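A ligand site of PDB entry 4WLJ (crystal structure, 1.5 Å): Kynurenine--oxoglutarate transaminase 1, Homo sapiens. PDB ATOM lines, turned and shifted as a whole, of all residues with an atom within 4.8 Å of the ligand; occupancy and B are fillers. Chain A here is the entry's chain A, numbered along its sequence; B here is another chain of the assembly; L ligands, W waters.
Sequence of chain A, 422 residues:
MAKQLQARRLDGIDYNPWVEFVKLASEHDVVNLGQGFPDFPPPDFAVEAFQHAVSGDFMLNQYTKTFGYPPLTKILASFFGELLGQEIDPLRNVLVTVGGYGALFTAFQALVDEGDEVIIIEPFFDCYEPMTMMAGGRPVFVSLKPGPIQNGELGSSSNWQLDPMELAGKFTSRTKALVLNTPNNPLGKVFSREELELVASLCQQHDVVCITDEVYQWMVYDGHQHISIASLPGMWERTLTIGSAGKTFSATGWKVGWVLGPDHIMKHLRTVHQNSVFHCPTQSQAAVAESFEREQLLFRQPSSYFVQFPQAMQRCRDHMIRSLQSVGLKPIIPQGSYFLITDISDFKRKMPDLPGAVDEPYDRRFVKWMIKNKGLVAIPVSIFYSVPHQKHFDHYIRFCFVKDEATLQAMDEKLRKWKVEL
An oxygen (O8) of the ligand lies within hydrogen-bond range of the backbone NH of Gly 100, at 2.8 Å.
O8 of the ligand sits at hydrogen-bond distance from OG of Ser 244.
The side-chain amide nitrogen of Asn 185 sits at hydrogen-bond distance from an oxygen (O1) of the ligand, at 2.8 Å.
An oxygen (O4) of the ligand is in salt-bridge range of the guanidinium group (NH1) of Arg 398.
The side-chain hydroxyl (OH) of Tyr 216 sits at hydrogen-bond distance from an oxygen (O1) of the ligand, 2.6 Å away.
An oxygen (O7) of the ligand is in salt-bridge range of the side-chain amino group of Lys 255, 2.8 Å away.
OD2 of Asp 213 sits at hydrogen-bond distance from N1 of the ligand, 2.7 Å away.
OH of Tyr 63 of chain B sits at hydrogen-bond distance from O6 of the ligand (2.6 Å).
O7 of the ligand is in hydrogen-bond range of N of Tyr 101 (2.9 Å).
The side-chain amide oxygen (OD1) of Asn 181 is in hydrogen-bond range of the backbone NH (N) of Asn 185 (3.1 Å).
O of Gly 34 sits at hydrogen-bond distance from NH2 of Arg 398, at 3.0 Å.
The side-chain carboxylate (OD2) of Asp 213 is in hydrogen-bond range of the side-chain hydroxyl (OH) of Tyr 128 (2.8 Å).
The backbone carbonyl oxygen (O) of Lys 255 sits at hydrogen-bond distance from the backbone NH (N) of Gly 99, at 3.2 Å.
OD1 of Asn 185 lies within hydrogen-bond range of NH1 of Arg 398 (2.9 Å).
OD1 of Asp 213 lies close to N of Val 215, 3.3 Å away.
NZ of Lys 247 sits at hydrogen-bond distance from OH of Tyr 63 of chain B, 3.2 Å away.
The backbone NH (N) of Tyr 63 of chain B lies within hydrogen-bond range of the side-chain hydroxyl (OG1) of Thr 252 (3.0 Å).
CA of Gly 36 touches O3 of the ligand, 3.6 Å away.
CA of Gly 99 touches O8 of the ligand (3.4 Å).
Phe 125 touches the ligand (CZ to C4, 3.4 Å).
OD1 of Asn 181 touches C2 of the ligand, at 3.5 Å.
Val 215 touches the ligand (CG2 to C1, 3.6 Å).
NZ of Lys 247 touches O2 of the ligand (3.5 Å).
Phe 339 touches the ligand (CZ to O3, 3.9 Å).
16 residues have an atom within 4 Å of the ligand: Gly 36, Gly 99, Gly 100, Tyr 101, Phe 125, Asn 181, Asn 185, Asp 213, Val 215, Tyr 216, Ser 244, Lys 247, Lys 255, Phe 339, Arg 398 and Tyr 63 of chain B.
The nearest printed residue that does not touch the ligand is Tyr 128 (4.04 Å).
Water W1 lies within hydrogen-bond range of O6 of the ligand (2.6 Å) and O of Thr 252 (2.7 Å).
Water W2 lies within hydrogen-bond range of O of Val 256 (2.9 Å), OG of Ser 244 (3.1 Å) and O8 of the ligand (3.1 Å).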
ATOM      1  N   GLY A  34     -16.521   4.580  -5.804  1.00  0.00           N
ATOM      2  CA  GLY A  34     -15.231   4.941  -6.368  1.00  0.00           C
ATOM      3  C   GLY A  34     -15.378   5.898  -7.536  1.00  0.00           C
ATOM      4  O   GLY A  34     -14.492   6.682  -7.794  1.00  0.00           O
ATOM      5  N   GLY A  36     -15.984   8.917  -9.642  1.00  0.00           N
ATOM      6  CA  GLY A  36     -16.102  10.362  -9.496  1.00  0.00           C
ATOM      7  C   GLY A  36     -17.119  11.016 -10.422  1.00  0.00           C
ATOM      8  O   GLY A  36     -16.827  11.972 -11.147  1.00  0.00           O
ATOM      9  N   VAL A  98     -11.447  19.934 -24.313  1.00  0.00           N
ATOM     10  CA  VAL A  98     -12.086  18.644 -24.071  1.00  0.00           C
ATOM     11  C   VAL A  98     -11.938  18.266 -22.582  1.00  0.00           C
ATOM     12  O   VAL A  98     -11.046  17.488 -22.118  1.00  0.00           O
ATOM     13  CB  VAL A  98     -11.487  17.534 -24.998  1.00  0.00           C
ATOM     14  CG1 VAL A  98     -12.166  16.174 -24.742  1.00  0.00           C
ATOM     15  CG2 VAL A  98     -11.597  17.940 -26.453  1.00  0.00           C
ATOM     16  N   GLY A  99     -12.807  18.878 -21.799  1.00  0.00           N
ATOM     17  CA  GLY A  99     -12.842  18.692 -20.372  1.00  0.00           C
ATOM     18  C   GLY A  99     -11.714  19.414 -19.665  1.00  0.00           C
ATOM     19  O   GLY A  99     -10.807  20.027 -20.253  1.00  0.00           O
ATOM     20  N   GLY A 100     -11.784  19.358 -18.350  1.00  0.00           N
ATOM     21  CA  GLY A 100     -10.639  19.716 -17.537  1.00  0.00           C
ATOM     22  C   GLY A 100      -9.373  18.946 -17.906  1.00  0.00           C
ATOM     23  O   GLY A 100      -8.273  19.479 -17.829  1.00  0.00           O
ATOM     24  N   TYR A 101      -9.504  17.660 -18.225  1.00  0.00           N
ATOM     25  CA  TYR A 101      -8.367  16.826 -18.648  1.00  0.00           C
ATOM     26  C   TYR A 101      -7.660  17.488 -19.815  1.00  0.00           C
ATOM     27  O   TYR A 101      -6.451  17.706 -19.795  1.00  0.00           O
ATOM     28  CB  TYR A 101      -8.793  15.406 -19.070  1.00  0.00           C
ATOM     29  CG  TYR A 101      -8.539  14.269 -18.092  1.00  0.00           C
ATOM     30  CD1 TYR A 101      -7.260  13.757 -17.889  1.00  0.00           C
ATOM     31  CD2 TYR A 101      -9.597  13.676 -17.407  1.00  0.00           C
ATOM     32  CE1 TYR A 101      -7.036  12.695 -16.986  1.00  0.00           C
ATOM     33  CE2 TYR A 101      -9.381  12.628 -16.509  1.00  0.00           C
ATOM     34  CZ  TYR A 101      -8.102  12.145 -16.307  1.00  0.00           C
ATOM     35  OH  TYR A 101      -7.913  11.083 -15.422  1.00  0.00           O
ATOM     36  N   LEU A 104      -5.803  20.657 -18.925  1.00  0.00           N
ATOM     37  CA  LEU A 104      -4.533  20.377 -18.263  1.00  0.00           C
ATOM     38  C   LEU A 104      -3.491  19.964 -19.302  1.00  0.00           C
ATOM     39  O   LEU A 104      -2.365  20.472 -19.299  1.00  0.00           O
ATOM     40  CB  LEU A 104      -4.708  19.271 -17.210  1.00  0.00           C
ATOM     41  CG  LEU A 104      -5.500  19.696 -15.958  1.00  0.00           C
ATOM     42  CD1 LEU A 104      -6.020  18.480 -15.264  1.00  0.00           C
ATOM     43  CD2 LEU A 104      -4.561  20.487 -15.032  1.00  0.00           C
ATOM     44  N   PHE A 125      -4.328  14.851  -8.037  1.00  0.00           N
ATOM     45  CA  PHE A 125      -5.064  14.234  -9.123  1.00  0.00           C
ATOM     46  C   PHE A 125      -4.043  13.594 -10.027  1.00  0.00           C
ATOM     47  O   PHE A 125      -3.086  14.258 -10.402  1.00  0.00           O
ATOM     48  CB  PHE A 125      -5.881  15.284  -9.849  1.00  0.00           C
ATOM     49  CG  PHE A 125      -6.724  14.745 -10.969  1.00  0.00           C
ATOM     50  CD1 PHE A 125      -7.693  13.814 -10.722  1.00  0.00           C
ATOM     51  CD2 PHE A 125      -6.565  15.241 -12.246  1.00  0.00           C
ATOM     52  CE1 PHE A 125      -8.483  13.315 -11.746  1.00  0.00           C
ATOM     53  CE2 PHE A 125      -7.347  14.755 -13.266  1.00  0.00           C
ATOM     54  CZ  PHE A 125      -8.304  13.774 -13.018  1.00  0.00           C
ATOM     55  N   TYR A 128      -1.363  14.638 -13.183  1.00  0.00           N
ATOM     56  CA  TYR A 128      -0.403  15.770 -13.215  1.00  0.00           C
ATOM     57  C   TYR A 128       1.010  15.224 -13.434  1.00  0.00           C
ATOM     58  O   TYR A 128       1.791  15.791 -14.146  1.00  0.00           O
ATOM     59  CB  TYR A 128      -0.411  16.617 -11.945  1.00  0.00           C
ATOM     60  CG  TYR A 128      -1.716  17.268 -11.565  1.00  0.00           C
ATOM     61  CD1 TYR A 128      -2.722  17.532 -12.506  1.00  0.00           C
ATOM     62  CD2 TYR A 128      -1.976  17.596 -10.254  1.00  0.00           C
ATOM     63  CE1 TYR A 128      -3.919  18.097 -12.116  1.00  0.00           C
ATOM     64  CE2 TYR A 128      -3.168  18.168  -9.853  1.00  0.00           C
ATOM     65  CZ  TYR A 128      -4.120  18.425 -10.790  1.00  0.00           C
ATOM     66  OH  TYR A 128      -5.307  18.970 -10.354  1.00  0.00           O
ATOM     67  N   ASN A 181      -4.536  22.509  -7.113  1.00  0.00           N
ATOM     68  CA  ASN A 181      -5.874  21.953  -7.317  1.00  0.00           C
ATOM     69  C   ASN A 181      -6.696  22.308  -6.092  1.00  0.00           C
ATOM     70  O   ASN A 181      -6.421  21.784  -5.008  1.00  0.00           O
ATOM     71  CB  ASN A 181      -5.776  20.441  -7.556  1.00  0.00           C
ATOM     72  CG  ASN A 181      -7.112  19.747  -7.673  1.00  0.00           C
ATOM     73  OD1 ASN A 181      -7.265  18.636  -7.219  1.00  0.00           O
ATOM     74  ND2 ASN A 181      -8.102  20.424  -8.229  1.00  0.00           N
ATOM     75  N   ASN A 185      -9.017  17.128  -5.165  1.00  0.00           N
ATOM     76  CA  ASN A 185      -9.232  15.682  -5.297  1.00  0.00           C
ATOM     77  C   ASN A 185      -7.872  15.038  -5.007  1.00  0.00           C
ATOM     78  O   ASN A 185      -6.903  15.342  -5.667  1.00  0.00           O
ATOM     79  CB  ASN A 185      -9.746  15.388  -6.715  1.00  0.00           C
ATOM     80  CG  ASN A 185      -9.853  13.916  -7.060  1.00  0.00           C
ATOM     81  OD1 ASN A 185      -9.697  13.030  -6.224  1.00  0.00           O
ATOM     82  ND2 ASN A 185     -10.166  13.639  -8.346  1.00  0.00           N
ATOM     83  N   ASP A 213      -6.213  24.194 -11.143  1.00  0.00           N
ATOM     84  CA  ASP A 213      -7.296  23.284 -11.446  1.00  0.00           C
ATOM     85  C   ASP A 213      -8.451  23.498 -10.469  1.00  0.00           C
ATOM     86  O   ASP A 213      -8.406  23.044  -9.307  1.00  0.00           O
ATOM     87  CB  ASP A 213      -6.780  21.843 -11.360  1.00  0.00           C
ATOM     88  CG  ASP A 213      -7.824  20.823 -11.740  1.00  0.00           C
ATOM     89  OD1 ASP A 213      -9.042  21.122 -11.751  1.00  0.00           O
ATOM     90  OD2 ASP A 213      -7.392  19.673 -12.004  1.00  0.00           O
ATOM     91  N   VAL A 215     -11.790  22.696 -10.964  1.00  0.00           N
ATOM     92  CA  VAL A 215     -12.990  22.067 -11.507  1.00  0.00           C
ATOM     93  C   VAL A 215     -14.095  21.894 -10.446  1.00  0.00           C
ATOM     94  O   VAL A 215     -15.270  21.888 -10.825  1.00  0.00           O
ATOM     95  CB  VAL A 215     -12.707  20.689 -12.183  1.00  0.00           C
ATOM     96  CG1 VAL A 215     -11.752  20.850 -13.390  1.00  0.00           C
ATOM     97  CG2 VAL A 215     -12.147  19.655 -11.191  1.00  0.00           C
ATOM     98  N   TYR A 216     -13.745  21.767  -9.161  1.00  0.00           N
ATOM     99  CA  TYR A 216     -14.735  21.601  -8.083  1.00  0.00           C
ATOM    100  C   TYR A 216     -15.129  22.903  -7.387  1.00  0.00           C
ATOM    101  O   TYR A 216     -15.678  22.858  -6.298  1.00  0.00           O
ATOM    102  CB  TYR A 216     -14.247  20.593  -6.993  1.00  0.00           C
ATOM    103  CG  TYR A 216     -14.023  19.220  -7.573  1.00  0.00           C
ATOM    104  CD1 TYR A 216     -15.093  18.424  -7.994  1.00  0.00           C
ATOM    105  CD2 TYR A 216     -12.730  18.747  -7.777  1.00  0.00           C
ATOM    106  CE1 TYR A 216     -14.865  17.165  -8.561  1.00  0.00           C
ATOM    107  CE2 TYR A 216     -12.495  17.515  -8.358  1.00  0.00           C
ATOM    108  CZ  TYR A 216     -13.574  16.734  -8.784  1.00  0.00           C
ATOM    109  OH  TYR A 216     -13.348  15.488  -9.369  1.00  0.00           O
ATOM    110  N   SER A 244     -14.427  22.809 -15.487  1.00  0.00           N
ATOM    111  CA  SER A 244     -15.037  21.657 -16.150  1.00  0.00           C
ATOM    112  C   SER A 244     -16.536  21.786 -16.111  1.00  0.00           C
ATOM    113  O   SER A 244     -17.115  21.925 -15.031  1.00  0.00           O
ATOM    114  CB  SER A 244     -14.638  20.350 -15.455  1.00  0.00           C
ATOM    115  OG  SER A 244     -15.433  19.265 -15.929  1.00  0.00           O
ATOM    116  N   LYS A 247     -18.198  18.844 -13.949  1.00  0.00           N
ATOM    117  CA  LYS A 247     -18.256  18.928 -12.500  1.00  0.00           C
ATOM    118  C   LYS A 247     -19.180  20.057 -12.063  1.00  0.00           C
ATOM    119  O   LYS A 247     -19.746  20.040 -10.984  1.00  0.00           O
ATOM    120  CB  LYS A 247     -16.862  19.125 -11.894  1.00  0.00           C
ATOM    121  CG  LYS A 247     -15.850  18.087 -12.331  1.00  0.00           C
ATOM    122  CD  LYS A 247     -16.335  16.673 -12.124  1.00  0.00           C
ATOM    123  CE  LYS A 247     -15.340  15.707 -12.708  1.00  0.00           C
ATOM    124  NZ  LYS A 247     -15.545  14.292 -12.257  1.00  0.00           N
ATOM    125  N   THR A 252     -20.795  14.627 -16.444  1.00  0.00           N
ATOM    126  CA  THR A 252     -19.353  14.377 -16.679  1.00  0.00           C
ATOM    127  C   THR A 252     -19.057  13.853 -18.081  1.00  0.00           C
ATOM    128  O   THR A 252     -17.937  14.020 -18.595  1.00  0.00           O
ATOM    129  CB  THR A 252     -18.778  13.386 -15.650  1.00  0.00           C
ATOM    130  OG1 THR A 252     -19.521  12.157 -15.670  1.00  0.00           O
ATOM    131  CG2 THR A 252     -18.811  13.977 -14.261  1.00  0.00           C
ATOM    132  N   LYS A 255     -17.855  16.278 -21.211  1.00  0.00           N
ATOM    133  CA  LYS A 255     -16.439  16.551 -21.470  1.00  0.00           C
ATOM    134  C   LYS A 255     -16.182  17.898 -22.176  1.00  0.00           C
ATOM    135  O   LYS A 255     -15.562  17.986 -23.231  1.00  0.00           O
ATOM    136  CB  LYS A 255     -15.820  15.383 -22.281  1.00  0.00           C
ATOM    137  CG  LYS A 255     -15.652  14.118 -21.507  1.00  0.00           C
ATOM    138  CD  LYS A 255     -14.619  14.243 -20.381  1.00  0.00           C
ATOM    139  CE  LYS A 255     -13.197  14.456 -20.895  1.00  0.00           C
ATOM    140  NZ  LYS A 255     -12.155  14.124 -19.869  1.00  0.00           N
ATOM    141  N   VAL A 256     -16.623  18.980 -21.517  1.00  0.00           N
ATOM    142  CA  VAL A 256     -16.337  20.359 -21.949  1.00  0.00           C
ATOM    143  C   VAL A 256     -15.621  21.036 -20.781  1.00  0.00           C
ATOM    144  O   VAL A 256     -16.095  20.992 -19.639  1.00  0.00           O
ATOM    145  CB  VAL A 256     -17.604  21.135 -22.270  1.00  0.00           C
ATOM    146  CG1 VAL A 256     -17.273  22.573 -22.635  1.00  0.00           C
ATOM    147  CG2 VAL A 256     -18.353  20.444 -23.438  1.00  0.00           C
ATOM    148  N   PHE A 339     -15.496  14.303  -2.870  1.00  0.00           N
ATOM    149  CA  PHE A 339     -14.804  13.196  -2.204  1.00  0.00           C
ATOM    150  C   PHE A 339     -14.490  13.438  -0.742  1.00  0.00           C
ATOM    151  O   PHE A 339     -14.430  14.575  -0.277  1.00  0.00           O
ATOM    152  CB  PHE A 339     -13.476  12.927  -2.924  1.00  0.00           C
ATOM    153  CG  PHE A 339     -13.625  12.803  -4.381  1.00  0.00           C
ATOM    154  CD1 PHE A 339     -14.237  11.698  -4.951  1.00  0.00           C
ATOM    155  CD2 PHE A 339     -13.126  13.794  -5.209  1.00  0.00           C
ATOM    156  CE1 PHE A 339     -14.379  11.598  -6.334  1.00  0.00           C
ATOM    157  CE2 PHE A 339     -13.268  13.695  -6.592  1.00  0.00           C
ATOM    158  CZ  PHE A 339     -13.895  12.590  -7.154  1.00  0.00           C
ATOM    159  N   PHE A 384      -2.616   8.730  -5.767  1.00  0.00           N
ATOM    160  CA  PHE A 384      -2.479  10.200  -5.771  1.00  0.00           C
ATOM    161  C   PHE A 384      -1.161  10.656  -5.105  1.00  0.00           C
ATOM    162  O   PHE A 384      -1.021  11.817  -4.712  1.00  0.00           O
ATOM    163  CB  PHE A 384      -3.697  10.828  -5.053  1.00  0.00           C
ATOM    164  CG  PHE A 384      -5.004  10.342  -5.609  1.00  0.00           C
ATOM    165  CD1 PHE A 384      -5.435  10.740  -6.869  1.00  0.00           C
ATOM    166  CD2 PHE A 384      -5.810   9.471  -4.886  1.00  0.00           C
ATOM    167  CE1 PHE A 384      -6.628  10.296  -7.385  1.00  0.00           C
ATOM    168  CE2 PHE A 384      -7.011   9.019  -5.429  1.00  0.00           C
ATOM    169  CZ  PHE A 384      -7.409   9.439  -6.666  1.00  0.00           C
ATOM    170  N   ARG A 398     -10.389   6.685  -0.715  1.00  0.00           N
ATOM    171  CA  ARG A 398     -11.250   7.783  -1.156  1.00  0.00           C
ATOM    172  C   ARG A 398     -12.624   7.312  -1.533  1.00  0.00           C
ATOM    173  O   ARG A 398     -12.778   6.374  -2.325  1.00  0.00           O
ATOM    174  CB  ARG A 398     -10.602   8.507  -2.364  1.00  0.00           C
ATOM    175  CG  ARG A 398     -11.345   9.809  -2.796  1.00  0.00           C
ATOM    176  CD  ARG A 398     -11.001  10.212  -4.196  1.00  0.00           C
ATOM    177  NE  ARG A 398     -11.772   9.431  -5.165  1.00  0.00           N
ATOM    178  CZ  ARG A 398     -11.677   9.585  -6.488  1.00  0.00           C
ATOM    179  NH1 ARG A 398     -10.850  10.487  -6.987  1.00  0.00           N
ATOM    180  NH2 ARG A 398     -12.399   8.825  -7.290  1.00  0.00           N
ATOM    181  N   TYR B  63     -19.621   9.968 -17.728  1.00  0.00           N
ATOM    182  CA  TYR B  63     -18.484   9.330 -18.375  1.00  0.00           C
ATOM    183  C   TYR B  63     -18.811   7.971 -18.972  1.00  0.00           C
ATOM    184  O   TYR B  63     -19.525   7.194 -18.366  1.00  0.00           O
ATOM    185  CB  TYR B  63     -17.367   9.110 -17.365  1.00  0.00           C
ATOM    186  CG  TYR B  63     -16.664  10.313 -16.801  1.00  0.00           C
ATOM    187  CD1 TYR B  63     -16.237  11.356 -17.597  1.00  0.00           C
ATOM    188  CD2 TYR B  63     -16.335  10.344 -15.455  1.00  0.00           C
ATOM    189  CE1 TYR B  63     -15.537  12.423 -17.067  1.00  0.00           C
ATOM    190  CE2 TYR B  63     -15.650  11.376 -14.939  1.00  0.00           C
ATOM    191  CZ  TYR B  63     -15.248  12.405 -15.731  1.00  0.00           C
ATOM    192  OH  TYR B  63     -14.534  13.446 -15.161  1.00  0.00           O
HETATM  193  N1  LIG L   1      -9.230  17.797 -12.441  1.00  0.00           N
HETATM  194  C1  LIG L   1      -9.659  17.091 -11.378  1.00  0.00           C
HETATM  195  C2  LIG L   1      -9.059  17.515 -10.042  1.00  0.00           C
HETATM  196  C3  LIG L   1     -10.550  16.043 -11.529  1.00  0.00           C
HETATM  197  O1  LIG L   1     -10.934  15.362 -10.357  1.00  0.00           O
HETATM  198  C4  LIG L   1     -11.064  15.700 -12.770  1.00  0.00           C
HETATM  199  C5  LIG L   1     -12.017  14.547 -12.908  1.00  0.00           C
HETATM  200  N2  LIG L   1     -11.894  13.610 -11.760  1.00  0.00           N
HETATM  201  O2  LIG L   1     -12.612  12.376 -11.895  1.00  0.00           O
HETATM  202  C6  LIG L   1     -11.731  11.257 -11.783  1.00  0.00           C
HETATM  203  C7  LIG L   1     -11.575  10.798 -10.374  1.00  0.00           C
HETATM  204  O3  LIG L   1     -12.555  10.134  -9.843  1.00  0.00           O
HETATM  205  O4  LIG L   1     -10.491  11.015  -9.750  1.00  0.00           O
HETATM  206  C8  LIG L   1     -10.636  16.433 -13.851  1.00  0.00           C
HETATM  207  C9  LIG L   1      -9.699  17.455 -13.659  1.00  0.00           C
HETATM  208  C10 LIG L   1     -11.069  16.180 -15.278  1.00  0.00           C
HETATM  209  O5  LIG L   1     -12.265  16.850 -15.581  1.00  0.00           O
HETATM  210  P1  LIG L   1     -13.062  16.542 -16.928  1.00  0.00           P
HETATM  211  O6  LIG L   1     -14.035  15.424 -16.736  1.00  0.00           O
HETATM  212  O7  LIG L   1     -12.039  16.241 -17.998  1.00  0.00           O
HETATM  213  O8  LIG L   1     -13.825  17.844 -17.187  1.00  0.00           O
HETATM  214  O   HOH W   1     -16.537  15.987 -17.313  1.00  0.00           O
HETATM  215  O   HOH W   2     -16.541  18.274 -18.626  1.00  0.00           O
